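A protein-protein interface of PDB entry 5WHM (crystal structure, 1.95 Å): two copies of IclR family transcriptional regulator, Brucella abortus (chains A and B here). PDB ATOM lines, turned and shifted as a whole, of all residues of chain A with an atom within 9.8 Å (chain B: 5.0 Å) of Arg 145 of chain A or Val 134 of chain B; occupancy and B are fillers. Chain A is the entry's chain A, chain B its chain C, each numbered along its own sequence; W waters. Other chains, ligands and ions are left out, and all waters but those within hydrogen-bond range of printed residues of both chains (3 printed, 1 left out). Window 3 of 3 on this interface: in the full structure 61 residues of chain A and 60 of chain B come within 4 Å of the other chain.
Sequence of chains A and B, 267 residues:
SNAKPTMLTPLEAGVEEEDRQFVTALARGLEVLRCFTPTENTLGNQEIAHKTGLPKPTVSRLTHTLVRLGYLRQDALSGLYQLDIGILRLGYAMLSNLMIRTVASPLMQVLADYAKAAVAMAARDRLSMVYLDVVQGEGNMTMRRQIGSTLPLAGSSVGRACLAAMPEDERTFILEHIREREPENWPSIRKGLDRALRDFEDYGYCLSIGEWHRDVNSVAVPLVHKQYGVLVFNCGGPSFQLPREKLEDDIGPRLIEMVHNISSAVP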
ATOM      1  N   PRO A  38      34.710  28.790  29.343  1.00  0.00           N
ATOM      2  CA  PRO A  38      33.829  29.963  29.257  1.00  0.00           C
ATOM      3  C   PRO A  38      33.972  30.922  30.435  1.00  0.00           C
ATOM      4  O   PRO A  38      33.977  32.144  30.233  1.00  0.00           O
ATOM      5  CB  PRO A  38      32.431  29.332  29.176  1.00  0.00           C
ATOM      6  CG  PRO A  38      32.667  28.044  28.465  1.00  0.00           C
ATOM      7  CD  PRO A  38      34.000  27.542  28.989  1.00  0.00           C
ATOM      8  N   LEU A  88      38.540  27.909  15.739  1.00  0.00           N
ATOM      9  CA  LEU A  88      37.218  27.653  15.186  1.00  0.00           C
ATOM     10  C   LEU A  88      37.341  26.998  13.820  1.00  0.00           C
ATOM     11  O   LEU A  88      36.555  26.113  13.455  1.00  0.00           O
ATOM     12  CB  LEU A  88      36.417  28.968  15.126  1.00  0.00           C
ATOM     13  CG  LEU A  88      34.933  28.878  14.795  1.00  0.00           C
ATOM     14  CD1 LEU A  88      34.191  28.325  16.006  1.00  0.00           C
ATOM     15  CD2 LEU A  88      34.379  30.303  14.460  1.00  0.00           C
ATOM     16  N   LEU A  95      34.441  18.711  12.347  1.00  0.00           N
ATOM     17  CA  LEU A  95      33.010  18.446  12.208  1.00  0.00           C
ATOM     18  C   LEU A  95      32.645  18.029  10.800  1.00  0.00           C
ATOM     19  O   LEU A  95      31.724  17.226  10.607  1.00  0.00           O
ATOM     20  CB  LEU A  95      32.189  19.679  12.612  1.00  0.00           C
ATOM     21  CG  LEU A  95      32.288  20.043  14.103  1.00  0.00           C
ATOM     22  CD1 LEU A  95      31.736  21.470  14.339  1.00  0.00           C
ATOM     23  CD2 LEU A  95      31.522  19.006  14.974  1.00  0.00           C
ATOM     24  N   TYR A 131      29.322  17.165  22.585  1.00  0.00           N
ATOM     25  CA  TYR A 131      28.249  17.275  21.586  1.00  0.00           C
ATOM     26  C   TYR A 131      28.800  17.564  20.189  1.00  0.00           C
ATOM     27  O   TYR A 131      29.552  18.517  19.996  1.00  0.00           O
ATOM     28  CB  TYR A 131      27.268  18.386  21.981  1.00  0.00           C
ATOM     29  CG  TYR A 131      26.205  17.932  22.999  1.00  0.00           C
ATOM     30  CD1 TYR A 131      26.107  16.604  23.395  1.00  0.00           C
ATOM     31  CD2 TYR A 131      25.248  18.809  23.463  1.00  0.00           C
ATOM     32  CE1 TYR A 131      25.112  16.178  24.317  1.00  0.00           C
ATOM     33  CE2 TYR A 131      24.245  18.395  24.355  1.00  0.00           C
ATOM     34  CZ  TYR A 131      24.191  17.079  24.780  1.00  0.00           C
ATOM     35  OH  TYR A 131      23.200  16.682  25.658  1.00  0.00           O
ATOM     36  N   ASP A 133      26.483  17.256  17.334  1.00  0.00           N
ATOM     37  CA  ASP A 133      25.354  17.768  16.560  1.00  0.00           C
ATOM     38  C   ASP A 133      24.164  17.798  17.504  1.00  0.00           C
ATOM     39  O   ASP A 133      24.017  16.889  18.341  1.00  0.00           O
ATOM     40  CB  ASP A 133      25.075  16.866  15.354  1.00  0.00           C
ATOM     41  CG  ASP A 133      24.162  17.549  14.312  1.00  0.00           C
ATOM     42  OD1 ASP A 133      24.063  18.800  14.313  1.00  0.00           O
ATOM     43  OD2 ASP A 133      23.539  16.822  13.527  1.00  0.00           O
ATOM     44  N   VAL A 134      23.390  18.871  17.450  1.00  0.00           N
ATOM     45  CA  VAL A 134      22.258  19.084  18.345  1.00  0.00           C
ATOM     46  C   VAL A 134      21.089  19.601  17.522  1.00  0.00           C
ATOM     47  O   VAL A 134      21.243  20.591  16.805  1.00  0.00           O
ATOM     48  CB  VAL A 134      22.591  20.094  19.463  1.00  0.00           C
ATOM     49  CG1 VAL A 134      21.419  20.170  20.431  1.00  0.00           C
ATOM     50  CG2 VAL A 134      23.854  19.671  20.220  1.00  0.00           C
ATOM     51  N   GLN A 136      16.892  20.846  17.972  1.00  0.00           N
ATOM     52  CA  GLN A 136      15.915  21.256  18.969  1.00  0.00           C
ATOM     53  C   GLN A 136      14.511  20.993  18.456  1.00  0.00           C
ATOM     54  O   GLN A 136      14.257  21.034  17.246  1.00  0.00           O
ATOM     55  CB  GLN A 136      16.063  22.745  19.322  1.00  0.00           C
ATOM     56  CG  GLN A 136      17.455  23.154  19.813  1.00  0.00           C
ATOM     57  CD  GLN A 136      17.721  22.691  21.245  1.00  0.00           C
ATOM     58  OE1 GLN A 136      18.869  22.526  21.645  1.00  0.00           O
ATOM     59  NE2 GLN A 136      16.655  22.504  22.022  1.00  0.00           N
ATOM     60  N   ASN A 140      11.957  25.991  19.979  1.00  0.00           N
ATOM     61  CA  ASN A 140      13.424  26.004  19.908  1.00  0.00           C
ATOM     62  C   ASN A 140      14.141  26.444  21.197  1.00  0.00           C
ATOM     63  O   ASN A 140      15.228  25.942  21.534  1.00  0.00           O
ATOM     64  CB  ASN A 140      13.846  26.897  18.725  1.00  0.00           C
ATOM     65  CG  ASN A 140      15.092  27.721  19.013  1.00  0.00           C
ATOM     66  OD1 ASN A 140      15.015  28.945  19.160  1.00  0.00           O
ATOM     67  ND2 ASN A 140      16.246  27.057  19.081  1.00  0.00           N
ATOM     68  N   THR A 142      19.368  27.833  22.704  1.00  0.00           N
ATOM     69  CA  THR A 142      18.868  29.165  22.345  1.00  0.00           C
ATOM     70  C   THR A 142      19.965  29.929  21.571  1.00  0.00           C
ATOM     71  O   THR A 142      20.528  29.359  20.622  1.00  0.00           O
ATOM     72  CB  THR A 142      18.396  29.927  23.607  1.00  0.00           C
ATOM     73  OG1 THR A 142      17.955  31.241  23.250  1.00  0.00           O
ATOM     74  CG2 THR A 142      19.508  29.982  24.682  1.00  0.00           C
ATOM     75  N   MET A 143      20.290  31.180  21.930  1.00  0.00           N
ATOM     76  CA  MET A 143      21.439  31.836  21.264  1.00  0.00           C
ATOM     77  C   MET A 143      22.777  31.077  21.508  1.00  0.00           C
ATOM     78  O   MET A 143      23.607  30.966  20.600  1.00  0.00           O
ATOM     79  CB  MET A 143      21.610  33.286  21.692  1.00  0.00           C
ATOM     80  CG  MET A 143      22.028  34.159  20.520  1.00  0.00           C
ATOM     81  SD  MET A 143      22.896  35.838  20.965  1.00  0.00           S
ATOM     82  CE  MET A 143      21.713  36.379  22.407  1.00  0.00           C
ATOM     83  N   ARG A 144      22.990  30.566  22.717  1.00  0.00           N
ATOM     84  CA  ARG A 144      24.225  29.822  22.978  1.00  0.00           C
ATOM     85  C   ARG A 144      24.296  28.578  22.104  1.00  0.00           C
ATOM     86  O   ARG A 144      23.394  27.736  22.128  1.00  0.00           O
ATOM     87  CB  ARG A 144      24.344  29.452  24.463  1.00  0.00           C
ATOM     88  CG  ARG A 144      25.608  28.568  24.756  1.00  0.00           C
ATOM     89  CD  ARG A 144      25.753  28.180  26.238  1.00  0.00           C
ATOM     90  NE  ARG A 144      24.739  27.221  26.684  1.00  0.00           N
ATOM     91  CZ  ARG A 144      24.885  25.885  26.729  1.00  0.00           C
ATOM     92  NH1 ARG A 144      26.019  25.277  26.350  1.00  0.00           N
ATOM     93  NH2 ARG A 144      23.873  25.143  27.165  1.00  0.00           N
ATOM     94  N   ARG A 145      25.372  28.448  21.339  1.00  0.00           N
ATOM     95  CA  ARG A 145      25.559  27.256  20.524  1.00  0.00           C
ATOM     96  C   ARG A 145      26.170  26.139  21.365  1.00  0.00           C
ATOM     97  O   ARG A 145      26.997  26.394  22.243  1.00  0.00           O
ATOM     98  CB  ARG A 145      26.436  27.575  19.302  1.00  0.00           C
ATOM     99  CG  ARG A 145      25.796  28.651  18.359  1.00  0.00           C
ATOM    100  CD  ARG A 145      26.676  28.957  17.139  1.00  0.00           C
ATOM    101  NE  ARG A 145      26.099  30.033  16.317  1.00  0.00           N
ATOM    102  CZ  ARG A 145      25.098  29.843  15.464  1.00  0.00           C
ATOM    103  NH1 ARG A 145      24.560  28.629  15.328  1.00  0.00           N
ATOM    104  NH2 ARG A 145      24.612  30.851  14.781  1.00  0.00           N
ATOM    105  N   GLN A 146      25.726  24.898  21.120  1.00  0.00           N
ATOM    106  CA  GLN A 146      26.089  23.781  21.976  1.00  0.00           C
ATOM    107  C   GLN A 146      27.017  22.781  21.327  1.00  0.00           C
ATOM    108  O   GLN A 146      27.454  21.864  22.010  1.00  0.00           O
ATOM    109  CB  GLN A 146      24.840  23.018  22.459  1.00  0.00           C
ATOM    110  CG  GLN A 146      23.916  23.840  23.317  1.00  0.00           C
ATOM    111  CD  GLN A 146      22.676  23.057  23.685  1.00  0.00           C
ATOM    112  OE1 GLN A 146      22.772  21.957  24.216  1.00  0.00           O
ATOM    113  NE2 GLN A 146      21.520  23.604  23.397  1.00  0.00           N
ATOM    114  N   ILE A 147      27.294  22.897  20.030  1.00  0.00           N
ATOM    115  CA  ILE A 147      28.221  21.963  19.397  1.00  0.00           C
ATOM    116  C   ILE A 147      29.616  22.206  19.959  1.00  0.00           C
ATOM    117  O   ILE A 147      30.065  23.353  20.102  1.00  0.00           O
ATOM    118  CB  ILE A 147      28.143  22.071  17.868  1.00  0.00           C
ATOM    119  CG1 ILE A 147      26.811  21.449  17.402  1.00  0.00           C
ATOM    120  CG2 ILE A 147      29.326  21.364  17.199  1.00  0.00           C
ATOM    121  CD1 ILE A 147      26.560  21.617  15.918  1.00  0.00           C
ATOM    122  N   GLY A 148      30.271  21.122  20.391  1.00  0.00           N
ATOM    123  CA  GLY A 148      31.526  21.218  21.102  1.00  0.00           C
ATOM    124  C   GLY A 148      31.422  21.430  22.596  1.00  0.00           C
ATOM    125  O   GLY A 148      32.458  21.499  23.269  1.00  0.00           O
ATOM    126  N   SER A 149      30.232  21.613  23.149  1.00  0.00           N
ATOM    127  CA  SER A 149      30.206  21.682  24.607  1.00  0.00           C
ATOM    128  C   SER A 149      30.323  20.267  25.190  1.00  0.00           C
ATOM    129  O   SER A 149      30.217  19.263  24.478  1.00  0.00           O
ATOM    130  CB  SER A 149      28.937  22.359  25.116  1.00  0.00           C
ATOM    131  OG  SER A 149      27.828  21.590  24.745  1.00  0.00           O
ATOM    132  N   THR A 150      30.575  20.188  26.502  1.00  0.00           N
ATOM    133  CA  THR A 150      30.961  18.920  27.105  1.00  0.00           C
ATOM    134  C   THR A 150      30.077  18.598  28.307  1.00  0.00           C
ATOM    135  O   THR A 150      29.499  19.486  28.933  1.00  0.00           O
ATOM    136  CB  THR A 150      32.429  18.934  27.561  1.00  0.00           C
ATOM    137  OG1 THR A 150      32.604  19.993  28.491  1.00  0.00           O
ATOM    138  CG2 THR A 150      33.388  19.135  26.401  1.00  0.00           C
ATOM    139  N   ALA B  93      33.551  25.518  20.910  1.00  0.00           N
ATOM    140  CA  ALA B  93      32.275  26.041  21.431  1.00  0.00           C
ATOM    141  C   ALA B  93      32.401  27.466  21.988  1.00  0.00           C
ATOM    142  O   ALA B  93      31.516  28.308  21.797  1.00  0.00           O
ATOM    143  CB  ALA B  93      31.725  25.095  22.496  1.00  0.00           C
ATOM    144  N   SER B  96      32.477  29.859  19.122  1.00  0.00           N
ATOM    145  CA  SER B  96      31.169  30.001  18.492  1.00  0.00           C
ATOM    146  C   SER B  96      30.238  30.871  19.322  1.00  0.00           C
ATOM    147  O   SER B  96      29.124  31.159  18.883  1.00  0.00           O
ATOM    148  CB  SER B  96      30.564  28.599  18.301  1.00  0.00           C
ATOM    149  OG  SER B  96      30.028  28.118  19.541  1.00  0.00           O
ATOM    150  N   ASN B  97      30.641  31.229  20.552  1.00  0.00           N
ATOM    151  CA  ASN B  97      29.783  31.941  21.501  1.00  0.00           C
ATOM    152  C   ASN B  97      30.429  33.229  21.989  1.00  0.00           C
ATOM    153  O   ASN B  97      30.275  33.608  23.147  1.00  0.00           O
ATOM    154  CB  ASN B  97      29.420  31.053  22.698  1.00  0.00           C
ATOM    155  CG  ASN B  97      28.435  29.956  22.315  1.00  0.00           C
ATOM    156  OD1 ASN B  97      27.408  30.227  21.695  1.00  0.00           O
ATOM    157  ND2 ASN B  97      28.749  28.711  22.672  1.00  0.00           N
ATOM    158  N   ARG B 101      28.292  38.553  20.000  1.00  0.00           N
ATOM    159  CA  ARG B 101      27.056  38.071  19.377  1.00  0.00           C
ATOM    160  C   ARG B 101      25.813  38.611  20.055  1.00  0.00           C
ATOM    161  O   ARG B 101      24.781  38.758  19.396  1.00  0.00           O
ATOM    162  CB  ARG B 101      26.965  36.539  19.380  1.00  0.00           C
ATOM    163  CG  ARG B 101      27.977  35.810  18.513  1.00  0.00           C
ATOM    164  CD  ARG B 101      27.791  34.275  18.702  1.00  0.00           C
ATOM    165  NE  ARG B 101      26.445  33.939  18.260  1.00  0.00           N
ATOM    166  CZ  ARG B 101      25.700  32.947  18.738  1.00  0.00           C
ATOM    167  NH1 ARG B 101      26.160  32.129  19.705  1.00  0.00           N
ATOM    168  NH2 ARG B 101      24.482  32.784  18.251  1.00  0.00           N
ATOM    169  N   MET B 108      21.907  41.949  13.231  1.00  0.00           N
ATOM    170  CA  MET B 108      22.110  41.214  11.986  1.00  0.00           C
ATOM    171  C   MET B 108      20.803  40.574  11.528  1.00  0.00           C
ATOM    172  O   MET B 108      20.536  40.449  10.329  1.00  0.00           O
ATOM    173  CB  MET B 108      23.197  40.140  12.168  1.00  0.00           C
ATOM    174  CG  MET B 108      24.595  40.723  12.304  1.00  0.00           C
ATOM    175  SD  MET B 108      25.891  39.448  13.135  1.00  0.00           S
ATOM    176  CE  MET B 108      25.805  37.978  11.861  1.00  0.00           C
ATOM    177  N   ALA B 118      21.409  36.309   3.785  1.00  0.00           N
ATOM    178  CA  ALA B 118      22.254  35.966   4.928  1.00  0.00           C
ATOM    179  C   ALA B 118      23.191  37.115   5.327  1.00  0.00           C
ATOM    180  O   ALA B 118      23.809  37.766   4.476  1.00  0.00           O
ATOM    181  CB  ALA B 118      23.069  34.713   4.611  1.00  0.00           C
ATOM    182  N   VAL B 119      23.294  37.359   6.633  1.00  0.00           N
ATOM    183  CA  VAL B 119      24.216  38.337   7.207  1.00  0.00           C
ATOM    184  C   VAL B 119      25.193  37.567   8.093  1.00  0.00           C
ATOM    185  O   VAL B 119      24.766  36.716   8.888  1.00  0.00           O
ATOM    186  CB  VAL B 119      23.470  39.423   8.004  1.00  0.00           C
ATOM    187  CG1 VAL B 119      24.409  40.406   8.669  1.00  0.00           C
ATOM    188  CG2 VAL B 119      22.466  40.190   7.048  1.00  0.00           C
ATOM    189  N   ALA B 120      26.493  37.836   7.928  1.00  0.00           N
ATOM    190  CA  ALA B 120      27.523  37.066   8.626  1.00  0.00           C
ATOM    191  C   ALA B 120      28.520  38.009   9.284  1.00  0.00           C
ATOM    192  O   ALA B 120      28.655  39.186   8.907  1.00  0.00           O
ATOM    193  CB  ALA B 120      28.261  36.084   7.683  1.00  0.00           C
ATOM    194  N   MET B 121      29.215  37.463  10.278  1.00  0.00           N
ATOM    195  CA  MET B 121      30.320  38.119  10.937  1.00  0.00           C
ATOM    196  C   MET B 121      31.572  37.212  10.807  1.00  0.00           C
ATOM    197  O   MET B 121      31.479  36.019  11.057  1.00  0.00           O
ATOM    198  CB  MET B 121      29.994  38.389  12.403  1.00  0.00           C
ATOM    199  CG  MET B 121      31.117  39.050  13.172  1.00  0.00           C
ATOM    200  SD  MET B 121      30.630  39.324  15.055  1.00  0.00           S
ATOM    201  CE  MET B 121      30.439  37.457  15.696  1.00  0.00           C
ATOM    202  N   TYR B 131      34.021  32.443   9.206  1.00  0.00           N
ATOM    203  CA  TYR B 131      32.705  32.869   9.702  1.00  0.00           C
ATOM    204  C   TYR B 131      32.555  32.571  11.208  1.00  0.00           C
ATOM    205  O   TYR B 131      32.622  31.408  11.625  1.00  0.00           O
ATOM    206  CB  TYR B 131      31.629  32.139   8.914  1.00  0.00           C
ATOM    207  CG  TYR B 131      31.165  32.848   7.644  1.00  0.00           C
ATOM    208  CD1 TYR B 131      31.873  33.911   7.099  1.00  0.00           C
ATOM    209  CD2 TYR B 131      29.982  32.483   7.047  1.00  0.00           C
ATOM    210  CE1 TYR B 131      31.416  34.566   5.951  1.00  0.00           C
ATOM    211  CE2 TYR B 131      29.520  33.120   5.923  1.00  0.00           C
ATOM    212  CZ  TYR B 131      30.239  34.152   5.370  1.00  0.00           C
ATOM    213  OH  TYR B 131      29.721  34.764   4.245  1.00  0.00           O
ATOM    214  N   LEU B 132      32.315  33.610  12.012  1.00  0.00           N
ATOM    215  CA  LEU B 132      32.065  33.468  13.447  1.00  0.00           C
ATOM    216  C   LEU B 132      30.585  33.345  13.770  1.00  0.00           C
ATOM    217  O   LEU B 132      30.216  32.725  14.789  1.00  0.00           O
ATOM    218  CB  LEU B 132      32.632  34.679  14.197  1.00  0.00           C
ATOM    219  CG  LEU B 132      34.032  35.107  13.742  1.00  0.00           C
ATOM    220  CD1 LEU B 132      34.493  36.427  14.402  1.00  0.00           C
ATOM    221  CD2 LEU B 132      34.999  33.965  14.069  1.00  0.00           C
ATOM    222  N   ASP B 133      29.734  33.919  12.924  1.00  0.00           N
ATOM    223  CA  ASP B 133      28.301  33.902  13.141  1.00  0.00           C
ATOM    224  C   ASP B 133      27.638  34.196  11.797  1.00  0.00           C
ATOM    225  O   ASP B 133      28.217  34.884  10.944  1.00  0.00           O
ATOM    226  CB  ASP B 133      27.843  34.902  14.225  1.00  0.00           C
ATOM    227  CG  ASP B 133      26.504  34.491  14.844  1.00  0.00           C
ATOM    228  OD1 ASP B 133      25.973  35.198  15.717  1.00  0.00           O
ATOM    229  OD2 ASP B 133      25.975  33.416  14.469  1.00  0.00           O
ATOM    230  N   VAL B 134      26.478  33.589  11.590  1.00  0.00           N
ATOM    231  CA  VAL B 134      25.689  33.720  10.367  1.00  0.00           C
ATOM    232  C   VAL B 134      24.232  33.727  10.784  1.00  0.00           C
ATOM    233  O   VAL B 134      23.798  32.866  11.559  1.00  0.00           O
ATOM    234  CB  VAL B 134      25.897  32.567   9.358  1.00  0.00           C
ATOM    235  CG1 VAL B 134      25.135  32.870   8.049  1.00  0.00           C
ATOM    236  CG2 VAL B 134      27.333  32.305   9.088  1.00  0.00           C
ATOM    237  N   VAL B 135      23.469  34.661  10.244  1.00  0.00           N
ATOM    238  CA  VAL B 135      22.041  34.759  10.495  1.00  0.00           C
ATOM    239  C   VAL B 135      21.351  34.842   9.147  1.00  0.00           C
ATOM    240  O   VAL B 135      21.797  35.583   8.265  1.00  0.00           O
ATOM    241  CB  VAL B 135      21.721  35.987  11.366  1.00  0.00           C
ATOM    242  CG1 VAL B 135      20.291  36.387  11.223  1.00  0.00           C
ATOM    243  CG2 VAL B 135      22.052  35.679  12.825  1.00  0.00           C
ATOM    244  N   GLN B 136      20.285  34.071   8.975  1.00  0.00           N
ATOM    245  CA  GLN B 136      19.507  34.091   7.749  1.00  0.00           C
ATOM    246  C   GLN B 136      18.185  34.803   7.973  1.00  0.00           C
ATOM    247  O   GLN B 136      17.573  34.692   9.047  1.00  0.00           O
ATOM    248  CB  GLN B 136      19.258  32.679   7.252  1.00  0.00           C
ATOM    249  CG  GLN B 136      20.536  32.006   6.917  1.00  0.00           C
ATOM    250  CD  GLN B 136      20.531  31.393   5.540  1.00  0.00           C
ATOM    251  OE1 GLN B 136      21.590  31.204   4.931  1.00  0.00           O
ATOM    252  NE2 GLN B 136      19.342  31.059   5.044  1.00  0.00           N
ATOM    253  N   ARG B 145      25.869  29.037   5.399  1.00  0.00           N
ATOM    254  CA  ARG B 145      27.293  28.762   5.571  1.00  0.00           C
ATOM    255  C   ARG B 145      27.579  28.510   7.052  1.00  0.00           C
ATOM    256  O   ARG B 145      26.925  29.066   7.939  1.00  0.00           O
ATOM    257  CB  ARG B 145      28.153  29.905   5.022  1.00  0.00           C
ATOM    258  CG  ARG B 145      28.076  30.009   3.477  1.00  0.00           C
ATOM    259  CD  ARG B 145      29.188  30.831   2.856  1.00  0.00           C
ATOM    260  NE  ARG B 145      30.519  30.300   3.133  1.00  0.00           N
ATOM    261  CZ  ARG B 145      31.115  29.338   2.427  1.00  0.00           C
ATOM    262  NH1 ARG B 145      30.493  28.777   1.392  1.00  0.00           N
ATOM    263  NH2 ARG B 145      32.341  28.932   2.768  1.00  0.00           N
ATOM    264  N   GLN B 146      28.532  27.644   7.320  1.00  0.00           N
ATOM    265  CA  GLN B 146      28.633  27.126   8.672  1.00  0.00           C
ATOM    266  C   GLN B 146      29.637  27.929   9.518  1.00  0.00           C
ATOM    267  O   GLN B 146      30.523  28.615   9.012  1.00  0.00           O
ATOM    268  CB  GLN B 146      29.034  25.649   8.630  1.00  0.00           C
ATOM    269  CG  GLN B 146      28.065  24.759   7.883  1.00  0.00           C
ATOM    270  CD  GLN B 146      26.783  24.578   8.663  1.00  0.00           C
ATOM    271  OE1 GLN B 146      26.810  24.044   9.771  1.00  0.00           O
ATOM    272  NE2 GLN B 146      25.657  25.047   8.111  1.00  0.00           N
ATOM    273  N   ILE B 147      29.495  27.792  10.836  1.00  0.00           N
ATOM    274  CA  ILE B 147      30.378  28.442  11.797  1.00  0.00           C
ATOM    275  C   ILE B 147      31.771  27.837  11.646  1.00  0.00           C
ATOM    276  O   ILE B 147      31.951  26.630  11.837  1.00  0.00           O
ATOM    277  CB  ILE B 147      29.843  28.238  13.228  1.00  0.00           C
ATOM    278  CG1 ILE B 147      28.384  28.688  13.318  1.00  0.00           C
ATOM    279  CG2 ILE B 147      30.707  28.959  14.263  1.00  0.00           C
ATOM    280  CD1 ILE B 147      28.202  30.135  13.016  1.00  0.00           C
HETATM  281  O   HOH W   1      22.380  30.462  17.718  1.00  0.00           O
HETATM  282  O   HOH W   2      34.446  23.046  22.222  1.00  0.00           O
HETATM  283  O   HOH W   3      29.022  25.617  18.916  1.00  0.00           O
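Of the 17 printed residues of chain A, 7 touch a printed residue of chain B. Hydrophobic or aromatic side chains of chain A that line the printed part of chain B: Leu 88 and Met 143. Printed residues of chain B that touch a printed residue of chain A: Ala 93, Ser 96, Asn 97, Arg 101, Tyr 131, Leu 132, Asp 133, Val 134 and Ile 147. Among the printed residues, 15 pairs touch across the chains.
Water W2 bridges the backbone carbonyl oxygen of Gly 148 of chain A and the backbone NH of Ala 93 of chain B. Water W3 lies within hydrogen-bond range of the backbone carbonyl oxygen of Ile 147 of chain A (2.8 Å) and the side-chain hydroxyl of Ser 96 of chain B (2.8 Å). Water W1 lies within hydrogen-bond range of O of Met 143 of chain A (3.2 Å) and NH2 of Arg 101 of chain B (3.2 Å).
Arg 145 of chain A touches six residues of chain B. Of chain A, only Arg 145 (3.9 Å) comes within 4 Å of Val 134 of chain B. Of chain A, only Arg 145 (2.9 Å) comes within 4 Å of Asp 133 of chain B. No residue of chain A comes within 4 Å of Val 135 of chain B. Of the printed residues of chain A, Tyr 131 of chain B touches Leu 88 (3.5 Å). Printed residues of chain B within 4 Å of Met 143 of chain A: Arg 101 (2.9 Å). The nearest residue of chain A that does not touch Val 134 of chain B is Leu 88 of chain A (9.0 Å). The nearest printed residue of chain B that does not touch Leu 88 of chain A is Ala 93 of chain B (5.7 Å).
Arg 145 of chain A touches Asp 133 of chain B, but with the chains exchanged Asp 133 of chain A does not touch Arg 145 of chain B (12.4 Å). Arg 145 of chain A touches Val 134 of chain B, but with the chains exchanged Val 134 of chain A does not touch Arg 145 of chain B (13.5 Å). Arg 145 of chain A touches Ile 147 of chain B, but with the chains exchanged Ile 147 of chain A does not touch Arg 145 of chain B (10.9 Å). 7 positions are printed for both chains.
Among the printed residues, merely in contact across the chains: Leu 88 of chain A with Ser 96 of chain B, Leu 88 of chain A with Tyr 131 of chain B, Leu 88 of chain A with Leu 132 of chain B, Leu 88 of chain A with Ile 147 of chain B, Arg 144 of chain A with Asn 97 of chain B, Arg 145 of chain A with Ser 96 of chain B, Arg 145 of chain A with Arg 101 of chain B, Arg 145 of chain A with Val 134 of chain B, Arg 145 of chain A with Ile 147 of chain B, Ile 147 of chain A with Ala 93 of chain B, Gly 148 of chain A with Ala 93 of chain B and Ser 149 of chain A with Ala 93 of chain B.
NH1 of Arg 101 of chain B lies within hydrogen-bond range of O of Met 143 of chain A (2.9 Å). The side-chain amide oxygen (OD1) of Asn 97 of chain B lies within hydrogen-bond range of the backbone NH (N) of Arg 145 of chain A (2.7 Å). NH2 of Arg 145 of chain A lies within salt-bridge range of OD2 of Asp 133 of chain B (2.9 Å).
The backbone NH (N) of Gly 148 of chain A lies within hydrogen-bond range of the backbone carbonyl oxygen (O) of Tyr 131 of chain A, at 2.7 Å. The backbone NH (N) of Tyr 131 of chain A sits at hydrogen-bond distance from the backbone carbonyl oxygen (O) of Ser 149 of chain A (3.0 Å). The backbone carbonyl oxygen (O) of Ala 93 of chain B sits at hydrogen-bond distance from the side-chain amide nitrogen (ND2) of Asn 97 of chain B (2.9 Å). OD1 of Asn 97 of chain B sits at hydrogen-bond distance from NH1 of Arg 101 of chain B (3.0 Å). The backbone carbonyl oxygen (O) of Met 121 of chain B sits at hydrogen-bond distance from the backbone NH (N) of Leu 132 of chain B, 2.7 Å away. O of Asp 133 of chain B sits at hydrogen-bond distance from N of Met 121 of chain B, 2.8 Å away.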
